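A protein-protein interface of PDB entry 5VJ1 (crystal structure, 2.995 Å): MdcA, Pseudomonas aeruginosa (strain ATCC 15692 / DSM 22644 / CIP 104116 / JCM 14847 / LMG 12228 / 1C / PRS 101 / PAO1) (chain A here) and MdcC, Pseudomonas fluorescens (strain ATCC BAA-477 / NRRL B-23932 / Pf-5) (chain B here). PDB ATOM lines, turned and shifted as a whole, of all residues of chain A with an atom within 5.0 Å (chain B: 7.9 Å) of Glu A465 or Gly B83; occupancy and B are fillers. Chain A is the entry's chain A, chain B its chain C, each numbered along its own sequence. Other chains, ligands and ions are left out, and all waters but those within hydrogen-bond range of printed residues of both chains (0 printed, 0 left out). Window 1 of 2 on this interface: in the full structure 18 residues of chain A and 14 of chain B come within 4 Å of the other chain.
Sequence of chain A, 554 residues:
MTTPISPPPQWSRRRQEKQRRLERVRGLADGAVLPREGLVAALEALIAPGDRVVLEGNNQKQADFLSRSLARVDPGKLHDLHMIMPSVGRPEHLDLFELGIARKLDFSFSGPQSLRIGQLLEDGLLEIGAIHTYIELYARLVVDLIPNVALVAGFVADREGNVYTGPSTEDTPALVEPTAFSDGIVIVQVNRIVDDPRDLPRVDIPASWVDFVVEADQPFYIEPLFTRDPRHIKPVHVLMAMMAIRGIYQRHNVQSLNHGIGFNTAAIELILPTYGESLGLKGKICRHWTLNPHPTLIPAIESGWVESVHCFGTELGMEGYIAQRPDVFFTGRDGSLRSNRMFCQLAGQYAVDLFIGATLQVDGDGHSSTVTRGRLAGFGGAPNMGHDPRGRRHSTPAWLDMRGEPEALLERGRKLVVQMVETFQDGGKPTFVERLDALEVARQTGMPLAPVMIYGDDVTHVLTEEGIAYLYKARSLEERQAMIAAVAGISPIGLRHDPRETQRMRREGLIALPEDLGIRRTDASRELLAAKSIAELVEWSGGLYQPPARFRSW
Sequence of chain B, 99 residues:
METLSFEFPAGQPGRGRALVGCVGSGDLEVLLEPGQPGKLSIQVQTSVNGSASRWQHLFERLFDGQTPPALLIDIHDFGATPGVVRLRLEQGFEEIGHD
Among the printed residues, pairs that only touch across the chains: Val A236 with Leu B87, Glu A422 with Gly B83, Glu A422 with Val B84, Glu A465 with Gly B83 and Arg A521 with Leu B87.
Of the 14 printed residues of chain A, 5 touch a printed residue of chain B. Of the 14 printed residues of chain B, 6 touch a printed residue of chain A. Hydrophobic or aromatic side chains of chain B that line the printed part of chain A: Val B84 and Leu B87. Among the printed residues, 9 pairs touch across the chains. Among the printed residues, Asp or Glu carboxylates within 4 Å of a Lys or Arg side-chain nitrogen of the other chain: Glu A466 with Arg B86 and Arg A521 with Glu B90.
Glu A465 touches just one residue of chain B: Gly B83. Of the printed residues of chain B, Val A236 touches Leu B87 (3.8 Å). Of the printed residues of chain A, Glu B90 touches Arg A521 (3.5 Å). Of the printed residues of chain A, Arg B86 touches Glu A466 (2.8 Å) and Arg A521 (3.3 Å). Of the printed residues of chain A, Thr B81 touches Glu A422. Leu B58 touches none of the printed residues of chain A. The nearest residue of chain B that does not touch Glu A465 is Pro B82 (4.7 Å). The nearest printed residue of chain A that does not touch Val B84 is Val A236 (4.01 Å).
N of Val B84 sits close to OG1 of Thr B81, 3.5 Å away. NE of Arg B86 is in salt-bridge range of OE1 of Glu B90, at 2.8 Å. The side-chain sulfur (SD) of Met A240 is in hydrogen-bond range of the backbone NH (N) of Glu A465, at 3.6 Å. The backbone carbonyl oxygen of Glu A465 lies within hydrogen-bond range of the guanidinium group of Arg A521, at 2.7 Å. The backbone NH (N) of Thr A423 is in hydrogen-bond range of the side-chain carboxylate (OE1) of Glu A465, at 2.9 Å.
NE of Arg A521 is in salt-bridge range of OE1 of Glu B90, at 3.8 Å. The side-chain carboxylate (OE2) of Glu A466 lies within salt-bridge range of the guanidinium group (NH1) of Arg B86. The guanidinium group of Arg A521 sits close to the guanidinium group of Arg B86 (3.3 Å). The side-chain carboxylate (OE1) of Glu A422 lies close to the side-chain hydroxyl (OG1) of Thr B81, at 2.4 Å.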
ATOM      1  N   VAL A 236      -6.598  -3.222 -16.836  1.00  0.00           N
ATOM      2  CA  VAL A 236      -6.939  -1.848 -16.406  1.00  0.00           C
ATOM      3  C   VAL A 236      -8.442  -1.766 -16.111  1.00  0.00           C
ATOM      4  O   VAL A 236      -8.867  -1.070 -15.191  1.00  0.00           O
ATOM      5  CB  VAL A 236      -6.538  -0.748 -17.464  1.00  0.00           C
ATOM      6  CG1 VAL A 236      -7.309  -0.923 -18.778  1.00  0.00           C
ATOM      7  CG2 VAL A 236      -6.742   0.657 -16.907  1.00  0.00           C
ATOM      8  N   LEU A 239      -9.062  -3.110 -12.850  1.00  0.00           N
ATOM      9  CA  LEU A 239      -8.650  -2.227 -11.756  1.00  0.00           C
ATOM     10  C   LEU A 239      -9.778  -1.275 -11.399  1.00  0.00           C
ATOM     11  O   LEU A 239     -10.025  -0.993 -10.227  1.00  0.00           O
ATOM     12  CB  LEU A 239      -7.391  -1.430 -12.099  1.00  0.00           C
ATOM     13  CG  LEU A 239      -7.009  -0.449 -10.977  1.00  0.00           C
ATOM     14  CD1 LEU A 239      -6.796  -1.129  -9.618  1.00  0.00           C
ATOM     15  CD2 LEU A 239      -5.797   0.387 -11.346  1.00  0.00           C
ATOM     16  N   MET A 240     -10.471  -0.782 -12.412  1.00  0.00           N
ATOM     17  CA  MET A 240     -11.588   0.105 -12.156  1.00  0.00           C
ATOM     18  C   MET A 240     -12.779  -0.670 -11.572  1.00  0.00           C
ATOM     19  O   MET A 240     -13.501  -0.162 -10.700  1.00  0.00           O
ATOM     20  CB  MET A 240     -11.980   0.845 -13.436  1.00  0.00           C
ATOM     21  CG  MET A 240     -10.823   1.623 -14.068  1.00  0.00           C
ATOM     22  SD  MET A 240     -11.278   2.713 -15.439  1.00  0.00           S
ATOM     23  CE  MET A 240     -11.408   1.538 -16.788  1.00  0.00           C
ATOM     24  N   MET A 243     -12.392  -0.862  -7.887  1.00  0.00           N
ATOM     25  CA  MET A 243     -12.654   0.397  -7.200  1.00  0.00           C
ATOM     26  C   MET A 243     -14.155   0.686  -7.179  1.00  0.00           C
ATOM     27  O   MET A 243     -14.668   1.261  -6.218  1.00  0.00           O
ATOM     28  CB  MET A 243     -11.907   1.554  -7.871  1.00  0.00           C
ATOM     29  CG  MET A 243     -10.418   1.316  -8.032  1.00  0.00           C
ATOM     30  SD  MET A 243      -9.570   2.629  -8.904  1.00  0.00           S
ATOM     31  CE  MET A 243      -9.251   3.541  -7.442  1.00  0.00           C
ATOM     32  N   VAL A 421     -14.599   5.745 -16.475  1.00  0.00           N
ATOM     33  CA  VAL A 421     -13.831   5.870 -17.693  1.00  0.00           C
ATOM     34  C   VAL A 421     -12.339   5.936 -17.407  1.00  0.00           C
ATOM     35  O   VAL A 421     -11.907   6.427 -16.362  1.00  0.00           O
ATOM     36  CB  VAL A 421     -14.277   7.124 -18.487  1.00  0.00           C
ATOM     37  CG1 VAL A 421     -13.618   8.369 -17.925  1.00  0.00           C
ATOM     38  CG2 VAL A 421     -13.945   6.981 -19.956  1.00  0.00           C
ATOM     39  N   GLU A 422     -11.559   5.413 -18.346  1.00  0.00           N
ATOM     40  CA  GLU A 422     -10.103   5.492 -18.305  1.00  0.00           C
ATOM     41  C   GLU A 422      -9.707   6.913 -18.688  1.00  0.00           C
ATOM     42  O   GLU A 422     -10.457   7.600 -19.384  1.00  0.00           O
ATOM     43  CB  GLU A 422      -9.495   4.458 -19.253  1.00  0.00           C
ATOM     44  CG  GLU A 422      -7.997   4.265 -19.182  1.00  0.00           C
ATOM     45  CD  GLU A 422      -7.548   3.063 -20.017  1.00  0.00           C
ATOM     46  OE1 GLU A 422      -6.329   2.881 -20.191  1.00  0.00           O
ATOM     47  OE2 GLU A 422      -8.413   2.319 -20.529  1.00  0.00           O
ATOM     48  N   THR A 423      -8.568   7.381 -18.190  1.00  0.00           N
ATOM     49  CA  THR A 423      -8.132   8.747 -18.452  1.00  0.00           C
ATOM     50  C   THR A 423      -7.965   8.980 -19.924  1.00  0.00           C
ATOM     51  O   THR A 423      -8.046  10.116 -20.389  1.00  0.00           O
ATOM     52  CB  THR A 423      -6.829   9.048 -17.777  1.00  0.00           C
ATOM     53  OG1 THR A 423      -5.957   7.924 -17.969  1.00  0.00           O
ATOM     54  CG2 THR A 423      -7.060   9.245 -16.322  1.00  0.00           C
ATOM     55  N   LEU A 463     -15.104   7.842 -11.808  1.00  0.00           N
ATOM     56  CA  LEU A 463     -14.248   6.669 -11.606  1.00  0.00           C
ATOM     57  C   LEU A 463     -13.270   6.435 -12.742  1.00  0.00           C
ATOM     58  O   LEU A 463     -13.659   6.259 -13.898  1.00  0.00           O
ATOM     59  CB  LEU A 463     -15.108   5.419 -11.389  1.00  0.00           C
ATOM     60  CG  LEU A 463     -14.463   4.038 -11.329  1.00  0.00           C
ATOM     61  CD1 LEU A 463     -13.326   4.006 -10.362  1.00  0.00           C
ATOM     62  CD2 LEU A 463     -15.543   3.071 -10.869  1.00  0.00           C
ATOM     63  N   THR A 464     -11.999   6.374 -12.364  1.00  0.00           N
ATOM     64  CA  THR A 464     -10.870   6.341 -13.282  1.00  0.00           C
ATOM     65  C   THR A 464      -9.856   5.284 -12.839  1.00  0.00           C
ATOM     66  O   THR A 464      -9.848   4.925 -11.666  1.00  0.00           O
ATOM     67  CB  THR A 464     -10.231   7.753 -13.332  1.00  0.00           C
ATOM     68  OG1 THR A 464     -11.078   8.627 -14.095  1.00  0.00           O
ATOM     69  CG2 THR A 464      -8.917   7.731 -13.962  1.00  0.00           C
ATOM     70  N   GLU A 465      -8.976   4.807 -13.727  1.00  0.00           N
ATOM     71  CA  GLU A 465      -7.894   3.921 -13.287  1.00  0.00           C
ATOM     72  C   GLU A 465      -6.980   4.668 -12.282  1.00  0.00           C
ATOM     73  O   GLU A 465      -6.157   4.067 -11.603  1.00  0.00           O
ATOM     74  CB  GLU A 465      -7.059   3.404 -14.475  1.00  0.00           C
ATOM     75  CG  GLU A 465      -5.918   4.348 -14.908  1.00  0.00           C
ATOM     76  CD  GLU A 465      -6.362   5.453 -15.869  1.00  0.00           C
ATOM     77  OE1 GLU A 465      -7.586   5.650 -16.025  1.00  0.00           O
ATOM     78  OE2 GLU A 465      -5.487   6.154 -16.433  1.00  0.00           O
ATOM     79  N   GLU A 466      -7.201   5.963 -12.117  1.00  0.00           N
ATOM     80  CA  GLU A 466      -6.393   6.762 -11.226  1.00  0.00           C
ATOM     81  C   GLU A 466      -6.952   6.694  -9.851  1.00  0.00           C
ATOM     82  O   GLU A 466      -6.202   6.743  -8.893  1.00  0.00           O
ATOM     83  CB  GLU A 466      -6.359   8.220 -11.657  1.00  0.00           C
ATOM     84  CG  GLU A 466      -5.463   8.517 -12.834  1.00  0.00           C
ATOM     85  CD  GLU A 466      -4.019   8.608 -12.419  1.00  0.00           C
ATOM     86  OE1 GLU A 466      -3.677   9.630 -11.771  1.00  0.00           O
ATOM     87  OE2 GLU A 466      -3.248   7.660 -12.745  1.00  0.00           O
ATOM     88  N   GLY A 467      -8.284   6.638  -9.760  1.00  0.00           N
ATOM     89  CA  GLY A 467      -8.993   6.687  -8.490  1.00  0.00           C
ATOM     90  C   GLY A 467     -10.445   7.137  -8.603  1.00  0.00           C
ATOM     91  O   GLY A 467     -10.986   7.286  -9.704  1.00  0.00           O
ATOM     92  N   PRO A 514      -6.647   3.813  -5.351  1.00  0.00           N
ATOM     93  CA  PRO A 514      -6.847   2.389  -5.094  1.00  0.00           C
ATOM     94  C   PRO A 514      -6.170   1.960  -3.794  1.00  0.00           C
ATOM     95  O   PRO A 514      -6.714   1.126  -3.076  1.00  0.00           O
ATOM     96  CB  PRO A 514      -6.251   1.724  -6.342  1.00  0.00           C
ATOM     97  CG  PRO A 514      -5.361   2.733  -6.914  1.00  0.00           C
ATOM     98  CD  PRO A 514      -6.021   4.038  -6.659  1.00  0.00           C
ATOM     99  N   ARG A 521      -2.702  -1.733  -6.832  1.00  0.00           N
ATOM    100  CA  ARG A 521      -2.914  -1.630  -8.271  1.00  0.00           C
ATOM    101  C   ARG A 521      -2.459  -2.869  -9.073  1.00  0.00           C
ATOM    102  O   ARG A 521      -3.127  -3.296 -10.022  1.00  0.00           O
ATOM    103  CB  ARG A 521      -2.204  -0.381  -8.803  1.00  0.00           C
ATOM    104  CG  ARG A 521      -2.376   0.856  -7.930  1.00  0.00           C
ATOM    105  CD  ARG A 521      -1.710   2.057  -8.559  1.00  0.00           C
ATOM    106  NE  ARG A 521      -2.285   2.323  -9.871  1.00  0.00           N
ATOM    107  CZ  ARG A 521      -3.027   3.388 -10.160  1.00  0.00           C
ATOM    108  NH1 ARG A 521      -3.243   4.325  -9.230  1.00  0.00           N
ATOM    109  NH2 ARG A 521      -3.516   3.533 -11.391  1.00  0.00           N
ATOM    110  N   LEU B  28       1.982  -2.852 -23.954  1.00  0.00           N
ATOM    111  CA  LEU B  28       3.397  -2.521 -24.092  1.00  0.00           C
ATOM    112  C   LEU B  28       4.233  -3.551 -23.347  1.00  0.00           C
ATOM    113  O   LEU B  28       3.734  -4.307 -22.518  1.00  0.00           O
ATOM    114  CB  LEU B  28       3.730  -1.121 -23.563  1.00  0.00           C
ATOM    115  CG  LEU B  28       3.789  -0.884 -22.047  1.00  0.00           C
ATOM    116  CD1 LEU B  28       4.446   0.442 -21.745  1.00  0.00           C
ATOM    117  CD2 LEU B  28       2.407  -0.926 -21.413  1.00  0.00           C
ATOM    118  N   LEU B  58       4.089  11.189 -17.481  1.00  0.00           N
ATOM    119  CA  LEU B  58       3.844   9.882 -16.907  1.00  0.00           C
ATOM    120  C   LEU B  58       4.964   9.535 -15.942  1.00  0.00           C
ATOM    121  O   LEU B  58       4.714   9.202 -14.789  1.00  0.00           O
ATOM    122  CB  LEU B  58       3.719   8.828 -18.001  1.00  0.00           C
ATOM    123  CG  LEU B  58       3.243   7.467 -17.493  1.00  0.00           C
ATOM    124  CD1 LEU B  58       2.039   7.624 -16.552  1.00  0.00           C
ATOM    125  CD2 LEU B  58       2.853   6.632 -18.678  1.00  0.00           C
ATOM    126  N   ALA B  80      -0.399   1.883 -26.222  1.00  0.00           N
ATOM    127  CA  ALA B  80      -1.092   1.636 -24.966  1.00  0.00           C
ATOM    128  C   ALA B  80      -1.455   2.969 -24.346  1.00  0.00           C
ATOM    129  O   ALA B  80      -0.703   3.938 -24.468  1.00  0.00           O
ATOM    130  CB  ALA B  80      -0.222   0.836 -24.018  1.00  0.00           C
ATOM    131  N   THR B  81      -2.601   3.026 -23.684  1.00  0.00           N
ATOM    132  CA  THR B  81      -3.021   4.244 -23.019  1.00  0.00           C
ATOM    133  C   THR B  81      -2.155   4.507 -21.820  1.00  0.00           C
ATOM    134  O   THR B  81      -1.666   3.549 -21.209  1.00  0.00           O
ATOM    135  CB  THR B  81      -4.447   4.139 -22.554  1.00  0.00           C
ATOM    136  OG1 THR B  81      -4.604   2.923 -21.813  1.00  0.00           O
ATOM    137  CG2 THR B  81      -5.365   4.120 -23.738  1.00  0.00           C
ATOM    138  N   PRO B  82      -1.966   5.796 -21.465  1.00  0.00           N
ATOM    139  CA  PRO B  82      -1.184   6.186 -20.281  1.00  0.00           C
ATOM    140  C   PRO B  82      -1.615   5.412 -19.020  1.00  0.00           C
ATOM    141  O   PRO B  82      -0.798   5.184 -18.120  1.00  0.00           O
ATOM    142  CB  PRO B  82      -1.492   7.667 -20.146  1.00  0.00           C
ATOM    143  CG  PRO B  82      -1.735   8.100 -21.528  1.00  0.00           C
ATOM    144  CD  PRO B  82      -2.491   6.980 -22.166  1.00  0.00           C
ATOM    145  N   GLY B  83      -2.877   4.984 -18.976  1.00  0.00           N
ATOM    146  CA  GLY B  83      -3.357   4.191 -17.863  1.00  0.00           C
ATOM    147  C   GLY B  83      -2.699   2.819 -17.848  1.00  0.00           C
ATOM    148  O   GLY B  83      -2.099   2.427 -16.844  1.00  0.00           O
ATOM    149  N   VAL B  84      -2.828   2.090 -18.964  1.00  0.00           N
ATOM    150  CA  VAL B  84      -2.204   0.774 -19.152  1.00  0.00           C
ATOM    151  C   VAL B  84      -0.698   0.870 -18.929  1.00  0.00           C
ATOM    152  O   VAL B  84      -0.115   0.024 -18.239  1.00  0.00           O
ATOM    153  CB  VAL B  84      -2.462   0.190 -20.564  1.00  0.00           C
ATOM    154  CG1 VAL B  84      -1.675  -1.062 -20.769  1.00  0.00           C
ATOM    155  CG2 VAL B  84      -3.920  -0.104 -20.758  1.00  0.00           C
ATOM    156  N   VAL B  85      -0.069   1.896 -19.514  1.00  0.00           N
ATOM    157  CA  VAL B  85       1.371   2.075 -19.370  1.00  0.00           C
ATOM    158  C   VAL B  85       1.740   2.161 -17.914  1.00  0.00           C
ATOM    159  O   VAL B  85       2.600   1.421 -17.453  1.00  0.00           O
ATOM    160  CB  VAL B  85       1.886   3.330 -20.093  1.00  0.00           C
ATOM    161  CG1 VAL B  85       3.392   3.435 -19.934  1.00  0.00           C
ATOM    162  CG2 VAL B  85       1.543   3.254 -21.555  1.00  0.00           C
ATOM    163  N   ARG B  86       1.094   3.084 -17.202  1.00  0.00           N
ATOM    164  CA  ARG B  86       1.390   3.313 -15.791  1.00  0.00           C
ATOM    165  C   ARG B  86       1.246   2.021 -15.000  1.00  0.00           C
ATOM    166  O   ARG B  86       2.038   1.725 -14.114  1.00  0.00           O
ATOM    167  CB  ARG B  86       0.482   4.395 -15.196  1.00  0.00           C
ATOM    168  CG  ARG B  86       0.616   4.445 -13.686  1.00  0.00           C
ATOM    169  CD  ARG B  86      -0.204   5.496 -12.948  1.00  0.00           C
ATOM    170  NE  ARG B  86       0.019   5.285 -11.519  1.00  0.00           N
ATOM    171  CZ  ARG B  86      -0.514   5.992 -10.532  1.00  0.00           C
ATOM    172  NH1 ARG B  86      -1.323   7.012 -10.787  1.00  0.00           N
ATOM    173  NH2 ARG B  86      -0.220   5.672  -9.278  1.00  0.00           N
ATOM    174  N   LEU B  87       0.218   1.255 -15.330  1.00  0.00           N
ATOM    175  CA  LEU B  87      -0.047   0.017 -14.649  1.00  0.00           C
ATOM    176  C   LEU B  87       1.127  -0.946 -14.842  1.00  0.00           C
ATOM    177  O   LEU B  87       1.599  -1.540 -13.871  1.00  0.00           O
ATOM    178  CB  LEU B  87      -1.344  -0.593 -15.169  1.00  0.00           C
ATOM    179  CG  LEU B  87      -2.049  -1.662 -14.341  1.00  0.00           C
ATOM    180  CD1 LEU B  87      -2.269  -1.195 -12.910  1.00  0.00           C
ATOM    181  CD2 LEU B  87      -3.358  -2.022 -15.008  1.00  0.00           C
ATOM    182  N   ARG B  88       1.619  -1.082 -16.075  1.00  0.00           N
ATOM    183  CA  ARG B  88       2.710  -2.037 -16.360  1.00  0.00           C
ATOM    184  C   ARG B  88       4.048  -1.605 -15.779  1.00  0.00           C
ATOM    185  O   ARG B  88       4.874  -2.439 -15.406  1.00  0.00           O
ATOM    186  CB  ARG B  88       2.877  -2.277 -17.865  1.00  0.00           C
ATOM    187  CG  ARG B  88       1.686  -3.017 -18.411  1.00  0.00           C
ATOM    188  CD  ARG B  88       1.970  -3.825 -19.629  1.00  0.00           C
ATOM    189  NE  ARG B  88       1.879  -5.239 -19.287  1.00  0.00           N
ATOM    190  CZ  ARG B  88       0.736  -5.898 -19.143  1.00  0.00           C
ATOM    191  NH1 ARG B  88      -0.413  -5.262 -19.318  1.00  0.00           N
ATOM    192  NH2 ARG B  88       0.744  -7.191 -18.826  1.00  0.00           N
ATOM    193  N   LEU B  89       4.277  -0.305 -15.718  1.00  0.00           N
ATOM    194  CA  LEU B  89       5.448   0.182 -15.022  1.00  0.00           C
ATOM    195  C   LEU B  89       5.428  -0.240 -13.543  1.00  0.00           C
ATOM    196  O   LEU B  89       6.456  -0.651 -12.998  1.00  0.00           O
ATOM    197  CB  LEU B  89       5.551   1.701 -15.180  1.00  0.00           C
ATOM    198  CG  LEU B  89       6.188   2.117 -16.505  1.00  0.00           C
ATOM    199  CD1 LEU B  89       5.998   3.582 -16.787  1.00  0.00           C
ATOM    200  CD2 LEU B  89       7.667   1.810 -16.394  1.00  0.00           C
ATOM    201  N   GLU B  90       4.262  -0.207 -12.906  1.00  0.00           N
ATOM    202  CA  GLU B  90       4.196  -0.576 -11.499  1.00  0.00           C
ATOM    203  C   GLU B  90       4.310  -2.077 -11.320  1.00  0.00           C
ATOM    204  O   GLU B  90       4.890  -2.541 -10.349  1.00  0.00           O
ATOM    205  CB  GLU B  90       2.914  -0.062 -10.884  1.00  0.00           C
ATOM    206  CG  GLU B  90       2.739   1.412 -11.099  1.00  0.00           C
ATOM    207  CD  GLU B  90       1.863   2.053 -10.056  1.00  0.00           C
ATOM    208  OE1 GLU B  90       1.358   3.175 -10.320  1.00  0.00           O
ATOM    209  OE2 GLU B  90       1.666   1.422  -8.985  1.00  0.00           O
ATOM    210  N   GLN B  91       3.734  -2.833 -12.244  1.00  0.00           N
ATOM    211  CA  GLN B  91       3.873  -4.279 -12.216  1.00  0.00           C
ATOM    212  C   GLN B  91       5.346  -4.595 -12.272  1.00  0.00           C
ATOM    213  O   GLN B  91       5.881  -5.352 -11.458  1.00  0.00           O
ATOM    214  CB  GLN B  91       3.157  -4.927 -13.392  1.00  0.00           C
ATOM    215  CG  GLN B  91       1.653  -4.703 -13.405  1.00  0.00           C
ATOM    216  CD  GLN B  91       0.999  -5.348 -14.617  1.00  0.00           C
ATOM    217  OE1 GLN B  91       0.037  -4.809 -15.197  1.00  0.00           O
ATOM    218  NE2 GLN B  91       1.541  -6.501 -15.029  1.00  0.00           N
